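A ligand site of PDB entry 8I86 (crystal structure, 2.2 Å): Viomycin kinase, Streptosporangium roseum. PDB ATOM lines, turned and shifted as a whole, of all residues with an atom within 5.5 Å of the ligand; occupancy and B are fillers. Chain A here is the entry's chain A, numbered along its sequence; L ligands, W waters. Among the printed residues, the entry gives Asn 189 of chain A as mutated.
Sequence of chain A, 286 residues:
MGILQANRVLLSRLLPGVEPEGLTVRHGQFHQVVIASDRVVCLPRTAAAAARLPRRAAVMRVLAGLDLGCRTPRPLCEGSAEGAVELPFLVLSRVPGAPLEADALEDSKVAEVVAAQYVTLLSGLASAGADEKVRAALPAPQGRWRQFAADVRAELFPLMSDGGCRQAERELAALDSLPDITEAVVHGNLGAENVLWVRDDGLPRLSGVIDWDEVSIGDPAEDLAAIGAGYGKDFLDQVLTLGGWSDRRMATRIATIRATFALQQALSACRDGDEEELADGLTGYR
The backbone NH of Gln 29 is in hydrogen-bond range of an oxygen (O2) of the ligand (3.2 Å). O of Val 95 lies within hydrogen-bond range of N4 of the ligand, at 2.9 Å. A ring nitrogen (ND1) of His 31 sits at hydrogen-bond distance from an oxygen (O6) of the ligand, at 2.8 Å. The side-chain carboxylate (OD1) of Asp 211 lies close to an oxygen (O3) of the ligand (2.8 Å). OD2 of Asp 213 sits close to O6 of the ligand (2.9 Å). An oxygen (O3) of the ligand sits close to the side-chain carboxylate (OE1) of Glu 214 (3.0 Å). The backbone NH (N) of Phe 30 sits at hydrogen-bond distance from an oxygen (O5) of the ligand (3.3 Å). N of His 31 is in hydrogen-bond range of O5 of the ligand (3.2 Å).
The side-chain carboxylate (OD2) of Asp 211 lies within hydrogen-bond range of the side-chain amide nitrogen (ND2) of Asn 189, at 3.1 Å. N of Ile 210 lies within hydrogen-bond range of O of Asn 194, at 3.0 Å. O of Arg 26 lies within hydrogen-bond range of N of Val 33, 3.0 Å away. The side-chain amide nitrogen of Asn 194 is in hydrogen-bond range of the side-chain carboxylate of Asp 211, at 3.3 Å. A ring nitrogen (ND1) of His 31 sits at hydrogen-bond distance from the side-chain carboxylate (OD2) of Asp 213, at 3.2 Å. The side-chain carboxylate (OE2) of Glu 214 lies close to the side-chain amide oxygen (OD1) of Asn 189, 3.3 Å away.
O of His 27 lies close to O10 of the ligand (3.2 Å). The backbone carbonyl oxygen of Ser 93 lies close to an oxygen (O14) of the ligand (2.9 Å). Residues that only touch the ligand: Arg 26 (3.6 Å), Gly 28 (3.3 Å), Val 33 (3.7 Å), Ile 35 (3.8 Å), Pro 73 (3.2 Å), Arg 94 (3.5 Å) and Ile 210 (3.7 Å). 16 residues have an atom within 4 Å of the ligand: Arg 26, His 27, Gly 28, Gln 29, Phe 30, His 31, Val 33, Ile 35, Pro 73, Ser 93, Arg 94, Val 95, Ile 210, Asp 211, Asp 213 and Glu 214. The nearest printed residue that does not touch the ligand is Val 40 (4.05 Å).
Water W2 lies within hydrogen-bond range of O2 of the ligand (2.6 Å) and OD2 of Asp 211 (3.4 Å).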
ATOM      1  N   ARG A  26     -24.481 -17.062  23.873  1.00  0.00           N
ATOM      2  CA  ARG A  26     -25.636 -17.950  23.784  1.00  0.00           C
ATOM      3  C   ARG A  26     -25.555 -18.961  24.919  1.00  0.00           C
ATOM      4  O   ARG A  26     -24.493 -19.168  25.498  1.00  0.00           O
ATOM      5  CB  ARG A  26     -25.706 -18.675  22.441  1.00  0.00           C
ATOM      6  CG  ARG A  26     -25.924 -17.773  21.237  1.00  0.00           C
ATOM      7  CD  ARG A  26     -27.323 -17.196  21.150  1.00  0.00           C
ATOM      8  NE  ARG A  26     -27.395 -16.139  20.149  1.00  0.00           N
ATOM      9  CZ  ARG A  26     -27.451 -14.825  20.396  1.00  0.00           C
ATOM     10  NH1 ARG A  26     -27.476 -14.367  21.636  1.00  0.00           N
ATOM     11  NH2 ARG A  26     -27.469 -13.972  19.387  1.00  0.00           N
ATOM     12  N   HIS A  27     -26.695 -19.595  25.212  1.00  0.00           N
ATOM     13  CA  HIS A  27     -26.823 -20.529  26.319  1.00  0.00           C
ATOM     14  C   HIS A  27     -27.098 -21.925  25.751  1.00  0.00           C
ATOM     15  O   HIS A  27     -26.837 -22.189  24.573  1.00  0.00           O
ATOM     16  CB  HIS A  27     -27.903 -20.021  27.289  1.00  0.00           C
ATOM     17  CG  HIS A  27     -27.617 -18.664  27.860  1.00  0.00           C
ATOM     18  ND1 HIS A  27     -27.236 -17.588  27.087  1.00  0.00           N
ATOM     19  CD2 HIS A  27     -27.641 -18.222  29.125  1.00  0.00           C
ATOM     20  CE1 HIS A  27     -27.043 -16.534  27.865  1.00  0.00           C
ATOM     21  NE2 HIS A  27     -27.283 -16.889  29.101  1.00  0.00           N
ATOM     22  N   GLY A  28     -27.586 -22.827  26.608  1.00  0.00           N
ATOM     23  CA  GLY A  28     -27.915 -24.185  26.205  1.00  0.00           C
ATOM     24  C   GLY A  28     -28.362 -25.014  27.399  1.00  0.00           C
ATOM     25  O   GLY A  28     -28.733 -24.454  28.435  1.00  0.00           O
ATOM     26  N   GLN A  29     -28.297 -26.338  27.263  1.00  0.00           N
ATOM     27  CA  GLN A  29     -28.712 -27.241  28.321  1.00  0.00           C
ATOM     28  C   GLN A  29     -27.583 -27.405  29.345  1.00  0.00           C
ATOM     29  O   GLN A  29     -27.846 -27.610  30.517  1.00  0.00           O
ATOM     30  CB  GLN A  29     -29.137 -28.585  27.736  1.00  0.00           C
ATOM     31  CG  GLN A  29     -29.982 -29.436  28.675  1.00  0.00           C
ATOM     32  CD  GLN A  29     -30.299 -30.824  28.160  1.00  0.00           C
ATOM     33  OE1 GLN A  29     -31.063 -31.559  28.767  1.00  0.00           O
ATOM     34  NE2 GLN A  29     -29.706 -31.197  27.036  1.00  0.00           N
ATOM     35  N   PHE A  30     -26.326 -27.316  28.880  1.00  0.00           N
ATOM     36  CA  PHE A  30     -25.170 -27.625  29.716  1.00  0.00           C
ATOM     37  C   PHE A  30     -24.078 -26.568  29.632  1.00  0.00           C
ATOM     38  O   PHE A  30     -23.225 -26.505  30.517  1.00  0.00           O
ATOM     39  CB  PHE A  30     -24.603 -29.003  29.337  1.00  0.00           C
ATOM     40  CG  PHE A  30     -25.601 -30.137  29.370  1.00  0.00           C
ATOM     41  CD1 PHE A  30     -25.782 -30.965  28.269  1.00  0.00           C
ATOM     42  CD2 PHE A  30     -26.368 -30.378  30.509  1.00  0.00           C
ATOM     43  CE1 PHE A  30     -26.699 -32.004  28.300  1.00  0.00           C
ATOM     44  CE2 PHE A  30     -27.286 -31.418  30.540  1.00  0.00           C
ATOM     45  CZ  PHE A  30     -27.445 -32.225  29.437  1.00  0.00           C
ATOM     46  N   HIS A  31     -24.073 -25.722  28.579  1.00  0.00           N
ATOM     47  CA  HIS A  31     -22.914 -24.890  28.305  1.00  0.00           C
ATOM     48  C   HIS A  31     -23.309 -23.444  28.012  1.00  0.00           C
ATOM     49  O   HIS A  31     -24.285 -23.195  27.304  1.00  0.00           O
ATOM     50  CB  HIS A  31     -22.116 -25.439  27.117  1.00  0.00           C
ATOM     51  CG  HIS A  31     -21.506 -26.773  27.363  1.00  0.00           C
ATOM     52  ND1 HIS A  31     -21.746 -27.865  26.560  1.00  0.00           N
ATOM     53  CD2 HIS A  31     -20.665 -27.196  28.318  1.00  0.00           C
ATOM     54  CE1 HIS A  31     -21.077 -28.903  27.021  1.00  0.00           C
ATOM     55  NE2 HIS A  31     -20.419 -28.528  28.096  1.00  0.00           N
ATOM     56  N   VAL A  33     -21.781 -20.402  25.874  1.00  0.00           N
ATOM     57  CA  VAL A  33     -20.907 -20.342  24.719  1.00  0.00           C
ATOM     58  C   VAL A  33     -20.675 -18.875  24.345  1.00  0.00           C
ATOM     59  O   VAL A  33     -21.619 -18.166  24.037  1.00  0.00           O
ATOM     60  CB  VAL A  33     -21.499 -21.150  23.542  1.00  0.00           C
ATOM     61  CG1 VAL A  33     -20.606 -21.103  22.313  1.00  0.00           C
ATOM     62  CG2 VAL A  33     -21.782 -22.597  23.925  1.00  0.00           C
ATOM     63  N   ILE A  35     -19.420 -16.195  21.735  1.00  0.00           N
ATOM     64  CA  ILE A  35     -19.341 -16.171  20.282  1.00  0.00           C
ATOM     65  C   ILE A  35     -18.371 -15.077  19.866  1.00  0.00           C
ATOM     66  O   ILE A  35     -18.624 -13.894  20.110  1.00  0.00           O
ATOM     67  CB  ILE A  35     -20.747 -15.972  19.678  1.00  0.00           C
ATOM     68  CG1 ILE A  35     -21.735 -17.065  20.103  1.00  0.00           C
ATOM     69  CG2 ILE A  35     -20.681 -15.847  18.166  1.00  0.00           C
ATOM     70  CD1 ILE A  35     -21.367 -18.457  19.631  1.00  0.00           C
ATOM     71  N   VAL A  40     -15.858 -20.128  18.985  1.00  0.00           N
ATOM     72  CA  VAL A  40     -16.652 -19.992  20.197  1.00  0.00           C
ATOM     73  C   VAL A  40     -15.850 -20.595  21.343  1.00  0.00           C
ATOM     74  O   VAL A  40     -14.973 -21.423  21.121  1.00  0.00           O
ATOM     75  CB  VAL A  40     -18.036 -20.655  20.049  1.00  0.00           C
ATOM     76  CG1 VAL A  40     -18.666 -20.315  18.705  1.00  0.00           C
ATOM     77  CG2 VAL A  40     -17.986 -22.157  20.227  1.00  0.00           C
ATOM     78  N   PRO A  73     -17.691 -28.163  14.086  1.00  0.00           N
ATOM     79  CA  PRO A  73     -16.876 -27.330  14.959  1.00  0.00           C
ATOM     80  C   PRO A  73     -15.601 -28.065  15.384  1.00  0.00           C
ATOM     81  O   PRO A  73     -15.663 -29.043  16.119  1.00  0.00           O
ATOM     82  CB  PRO A  73     -17.788 -27.047  16.164  1.00  0.00           C
ATOM     83  CG  PRO A  73     -19.179 -27.424  15.692  1.00  0.00           C
ATOM     84  CD  PRO A  73     -18.959 -28.558  14.720  1.00  0.00           C
ATOM     85  N   LEU A  92     -13.936 -24.001  20.024  1.00  0.00           N
ATOM     86  CA  LEU A  92     -14.345 -24.677  18.801  1.00  0.00           C
ATOM     87  C   LEU A  92     -14.404 -23.655  17.665  1.00  0.00           C
ATOM     88  O   LEU A  92     -14.701 -22.484  17.910  1.00  0.00           O
ATOM     89  CB  LEU A  92     -15.722 -25.305  19.015  1.00  0.00           C
ATOM     90  CG  LEU A  92     -15.820 -26.387  20.081  1.00  0.00           C
ATOM     91  CD1 LEU A  92     -17.275 -26.766  20.339  1.00  0.00           C
ATOM     92  CD2 LEU A  92     -15.030 -27.626  19.691  1.00  0.00           C
ATOM     93  N   SER A  93     -14.142 -24.102  16.433  1.00  0.00           N
ATOM     94  CA  SER A  93     -14.328 -23.265  15.259  1.00  0.00           C
ATOM     95  C   SER A  93     -15.800 -22.916  15.108  1.00  0.00           C
ATOM     96  O   SER A  93     -16.671 -23.705  15.495  1.00  0.00           O
ATOM     97  CB  SER A  93     -13.792 -23.920  13.994  1.00  0.00           C
ATOM     98  OG  SER A  93     -14.418 -25.181  13.749  1.00  0.00           O
ATOM     99  N   ARG A  94     -16.073 -21.721  14.582  1.00  0.00           N
ATOM    100  CA  ARG A  94     -17.410 -21.326  14.198  1.00  0.00           C
ATOM    101  C   ARG A  94     -17.658 -21.722  12.750  1.00  0.00           C
ATOM    102  O   ARG A  94     -17.046 -21.161  11.835  1.00  0.00           O
ATOM    103  CB  ARG A  94     -17.647 -19.816  14.279  1.00  0.00           C
ATOM    104  CG  ARG A  94     -18.286 -19.372  15.580  1.00  0.00           C
ATOM    105  CD  ARG A  94     -18.676 -17.912  15.530  1.00  0.00           C
ATOM    106  NE  ARG A  94     -19.868 -17.613  14.758  1.00  0.00           N
ATOM    107  CZ  ARG A  94     -20.354 -16.384  14.575  1.00  0.00           C
ATOM    108  NH1 ARG A  94     -19.695 -15.329  15.026  1.00  0.00           N
ATOM    109  NH2 ARG A  94     -21.498 -16.201  13.939  1.00  0.00           N
ATOM    110  N   VAL A  95     -18.553 -22.687  12.564  1.00  0.00           N
ATOM    111  CA  VAL A  95     -19.093 -23.007  11.264  1.00  0.00           C
ATOM    112  C   VAL A  95     -19.806 -21.773  10.715  1.00  0.00           C
ATOM    113  O   VAL A  95     -20.703 -21.234  11.366  1.00  0.00           O
ATOM    114  CB  VAL A  95     -20.054 -24.205  11.381  1.00  0.00           C
ATOM    115  CG1 VAL A  95     -20.719 -24.525  10.051  1.00  0.00           C
ATOM    116  CG2 VAL A  95     -19.337 -25.427  11.936  1.00  0.00           C
ATOM    117  N   PRO A  96     -19.420 -21.273   9.515  1.00  0.00           N
ATOM    118  CA  PRO A  96     -20.106 -20.128   8.916  1.00  0.00           C
ATOM    119  C   PRO A  96     -21.450 -20.517   8.310  1.00  0.00           C
ATOM    120  O   PRO A  96     -21.709 -21.698   8.086  1.00  0.00           O
ATOM    121  CB  PRO A  96     -19.130 -19.666   7.823  1.00  0.00           C
ATOM    122  CG  PRO A  96     -18.402 -20.920   7.420  1.00  0.00           C
ATOM    123  CD  PRO A  96     -18.321 -21.766   8.679  1.00  0.00           C
ATOM    124  N   ASN A 189     -30.210 -33.963  17.188  1.00  0.00           N
ATOM    125  CA  ASN A 189     -30.825 -32.666  17.358  1.00  0.00           C
ATOM    126  C   ASN A 189     -30.798 -31.909  16.031  1.00  0.00           C
ATOM    127  O   ASN A 189     -30.592 -30.691  16.024  1.00  0.00           O
ATOM    128  CB  ASN A 189     -30.118 -31.905  18.477  1.00  0.00           C
ATOM    129  CG  ASN A 189     -31.022 -30.933  19.213  1.00  0.00           C
ATOM    130  OD1 ASN A 189     -32.055 -31.348  19.737  1.00  0.00           O
ATOM    131  ND2 ASN A 189     -30.648 -29.670  19.252  1.00  0.00           N
ATOM    132  N   ASN A 194     -29.604 -25.974  13.380  1.00  0.00           N
ATOM    133  CA  ASN A 194     -28.271 -26.517  13.559  1.00  0.00           C
ATOM    134  C   ASN A 194     -27.609 -26.894  12.232  1.00  0.00           C
ATOM    135  O   ASN A 194     -26.526 -27.479  12.236  1.00  0.00           O
ATOM    136  CB  ASN A 194     -28.285 -27.746  14.467  1.00  0.00           C
ATOM    137  CG  ASN A 194     -28.633 -27.419  15.900  1.00  0.00           C
ATOM    138  OD1 ASN A 194     -28.198 -26.381  16.418  1.00  0.00           O
ATOM    139  ND2 ASN A 194     -29.393 -28.278  16.552  1.00  0.00           N
ATOM    140  N   LEU A 196     -26.256 -25.211   8.704  1.00  0.00           N
ATOM    141  CA  LEU A 196     -25.882 -23.885   8.246  1.00  0.00           C
ATOM    142  C   LEU A 196     -25.473 -23.942   6.774  1.00  0.00           C
ATOM    143  O   LEU A 196     -24.846 -24.911   6.341  1.00  0.00           O
ATOM    144  CB  LEU A 196     -24.727 -23.364   9.119  1.00  0.00           C
ATOM    145  CG  LEU A 196     -24.956 -23.434  10.631  1.00  0.00           C
ATOM    146  CD1 LEU A 196     -23.853 -22.704  11.374  1.00  0.00           C
ATOM    147  CD2 LEU A 196     -26.312 -22.852  11.009  1.00  0.00           C
ATOM    148  N   ILE A 210     -23.847 -27.977  13.595  1.00  0.00           N
ATOM    149  CA  ILE A 210     -23.417 -27.623  14.941  1.00  0.00           C
ATOM    150  C   ILE A 210     -24.305 -28.338  15.964  1.00  0.00           C
ATOM    151  O   ILE A 210     -25.226 -29.056  15.582  1.00  0.00           O
ATOM    152  CB  ILE A 210     -23.433 -26.093  15.137  1.00  0.00           C
ATOM    153  CG1 ILE A 210     -24.859 -25.529  15.089  1.00  0.00           C
ATOM    154  CG2 ILE A 210     -22.530 -25.415  14.126  1.00  0.00           C
ATOM    155  CD1 ILE A 210     -24.936 -24.028  15.253  1.00  0.00           C
ATOM    156  N   ASP A 211     -23.988 -28.143  17.249  1.00  0.00           N
ATOM    157  CA  ASP A 211     -24.809 -28.584  18.365  1.00  0.00           C
ATOM    158  C   ASP A 211     -24.828 -30.106  18.444  1.00  0.00           C
ATOM    159  O   ASP A 211     -25.878 -30.741  18.322  1.00  0.00           O
ATOM    160  CB  ASP A 211     -26.213 -27.974  18.287  1.00  0.00           C
ATOM    161  CG  ASP A 211     -27.047 -28.168  19.539  1.00  0.00           C
ATOM    162  OD1 ASP A 211     -26.542 -28.776  20.502  1.00  0.00           O
ATOM    163  OD2 ASP A 211     -28.209 -27.706  19.543  1.00  0.00           O
ATOM    164  N   ASP A 213     -24.092 -31.965  21.093  1.00  0.00           N
ATOM    165  CA  ASP A 213     -24.027 -32.390  22.489  1.00  0.00           C
ATOM    166  C   ASP A 213     -24.857 -33.657  22.704  1.00  0.00           C
ATOM    167  O   ASP A 213     -24.554 -34.427  23.604  1.00  0.00           O
ATOM    168  CB  ASP A 213     -24.457 -31.279  23.442  1.00  0.00           C
ATOM    169  CG  ASP A 213     -23.551 -30.058  23.347  1.00  0.00           C
ATOM    170  OD1 ASP A 213     -23.675 -29.322  22.334  1.00  0.00           O
ATOM    171  OD2 ASP A 213     -22.712 -29.878  24.261  1.00  0.00           O
ATOM    172  N   GLU A 214     -25.873 -33.882  21.862  1.00  0.00           N
ATOM    173  CA  GLU A 214     -26.742 -35.031  22.005  1.00  0.00           C
ATOM    174  C   GLU A 214     -26.353 -36.147  21.038  1.00  0.00           C
ATOM    175  O   GLU A 214     -27.161 -37.022  20.769  1.00  0.00           O
ATOM    176  CB  GLU A 214     -28.187 -34.581  21.786  1.00  0.00           C
ATOM    177  CG  GLU A 214     -28.670 -33.614  22.851  1.00  0.00           C
ATOM    178  CD  GLU A 214     -29.570 -32.517  22.318  1.00  0.00           C
ATOM    179  OE1 GLU A 214     -29.048 -31.624  21.628  1.00  0.00           O
ATOM    180  OE2 GLU A 214     -30.793 -32.582  22.571  1.00  0.00           O
HETATM  181  P1  LIG L   1     -26.929 -28.750  24.202  1.00  0.00           P
HETATM  182  O1  LIG L   1     -26.414 -29.462  25.429  1.00  0.00           O
HETATM  183  O2  LIG L   1     -28.127 -27.862  24.487  1.00  0.00           O
HETATM  184  O3  LIG L   1     -27.193 -29.702  23.054  1.00  0.00           O
HETATM  185  O4  LIG L   1     -25.757 -27.740  23.728  1.00  0.00           O
HETATM  186  P2  LIG L   1     -24.835 -26.661  24.477  1.00  0.00           P
HETATM  187  O5  LIG L   1     -25.446 -26.344  25.801  1.00  0.00           O
HETATM  188  O6  LIG L   1     -23.401 -27.082  24.412  1.00  0.00           O
HETATM  189  O7  LIG L   1     -24.984 -25.386  23.524  1.00  0.00           O
HETATM  190  P3  LIG L   1     -25.202 -25.193  21.944  1.00  0.00           P
HETATM  191  O8  LIG L   1     -23.878 -25.257  21.240  1.00  0.00           O
HETATM  192  O9  LIG L   1     -26.270 -26.115  21.482  1.00  0.00           O
HETATM  193  O10 LIG L   1     -25.760 -23.693  21.933  1.00  0.00           O
HETATM  194  C1  LIG L   1     -24.869 -22.560  21.862  1.00  0.00           C
HETATM  195  C2  LIG L   1     -25.222 -21.749  20.639  1.00  0.00           C
HETATM  196  O11 LIG L   1     -24.041 -21.064  20.169  1.00  0.00           O
HETATM  197  C3  LIG L   1     -25.720 -22.549  19.427  1.00  0.00           C
HETATM  198  O12 LIG L   1     -27.120 -22.790  19.484  1.00  0.00           O
HETATM  199  C4  LIG L   1     -25.332 -21.621  18.286  1.00  0.00           C
HETATM  200  O13 LIG L   1     -26.206 -20.515  18.135  1.00  0.00           O
HETATM  201  C5  LIG L   1     -23.958 -21.163  18.762  1.00  0.00           C
HETATM  202  N1  LIG L   1     -22.873 -22.095  18.427  1.00  0.00           N
HETATM  203  C6  LIG L   1     -22.392 -23.126  19.193  1.00  0.00           C
HETATM  204  N2  LIG L   1     -21.410 -23.781  18.615  1.00  0.00           N
HETATM  205  C7  LIG L   1     -21.250 -23.141  17.394  1.00  0.00           C
HETATM  206  C8  LIG L   1     -20.328 -23.386  16.345  1.00  0.00           C
HETATM  207  O14 LIG L   1     -19.460 -24.268  16.274  1.00  0.00           O
HETATM  208  N3  LIG L   1     -20.513 -22.497  15.285  1.00  0.00           N
HETATM  209  C9  LIG L   1     -21.438 -21.485  15.245  1.00  0.00           C
HETATM  210  N4  LIG L   1     -21.464 -20.731  14.135  1.00  0.00           N
HETATM  211  N5  LIG L   1     -22.297 -21.238  16.240  1.00  0.00           N
HETATM  212  C10 LIG L   1     -22.136 -22.092  17.271  1.00  0.00           C
HETATM  213  O   HOH W   1     -21.330 -26.431  22.878  1.00  0.00           O
HETATM  214  O   HOH W   2     -29.031 -26.296  22.566  1.00  0.00           O
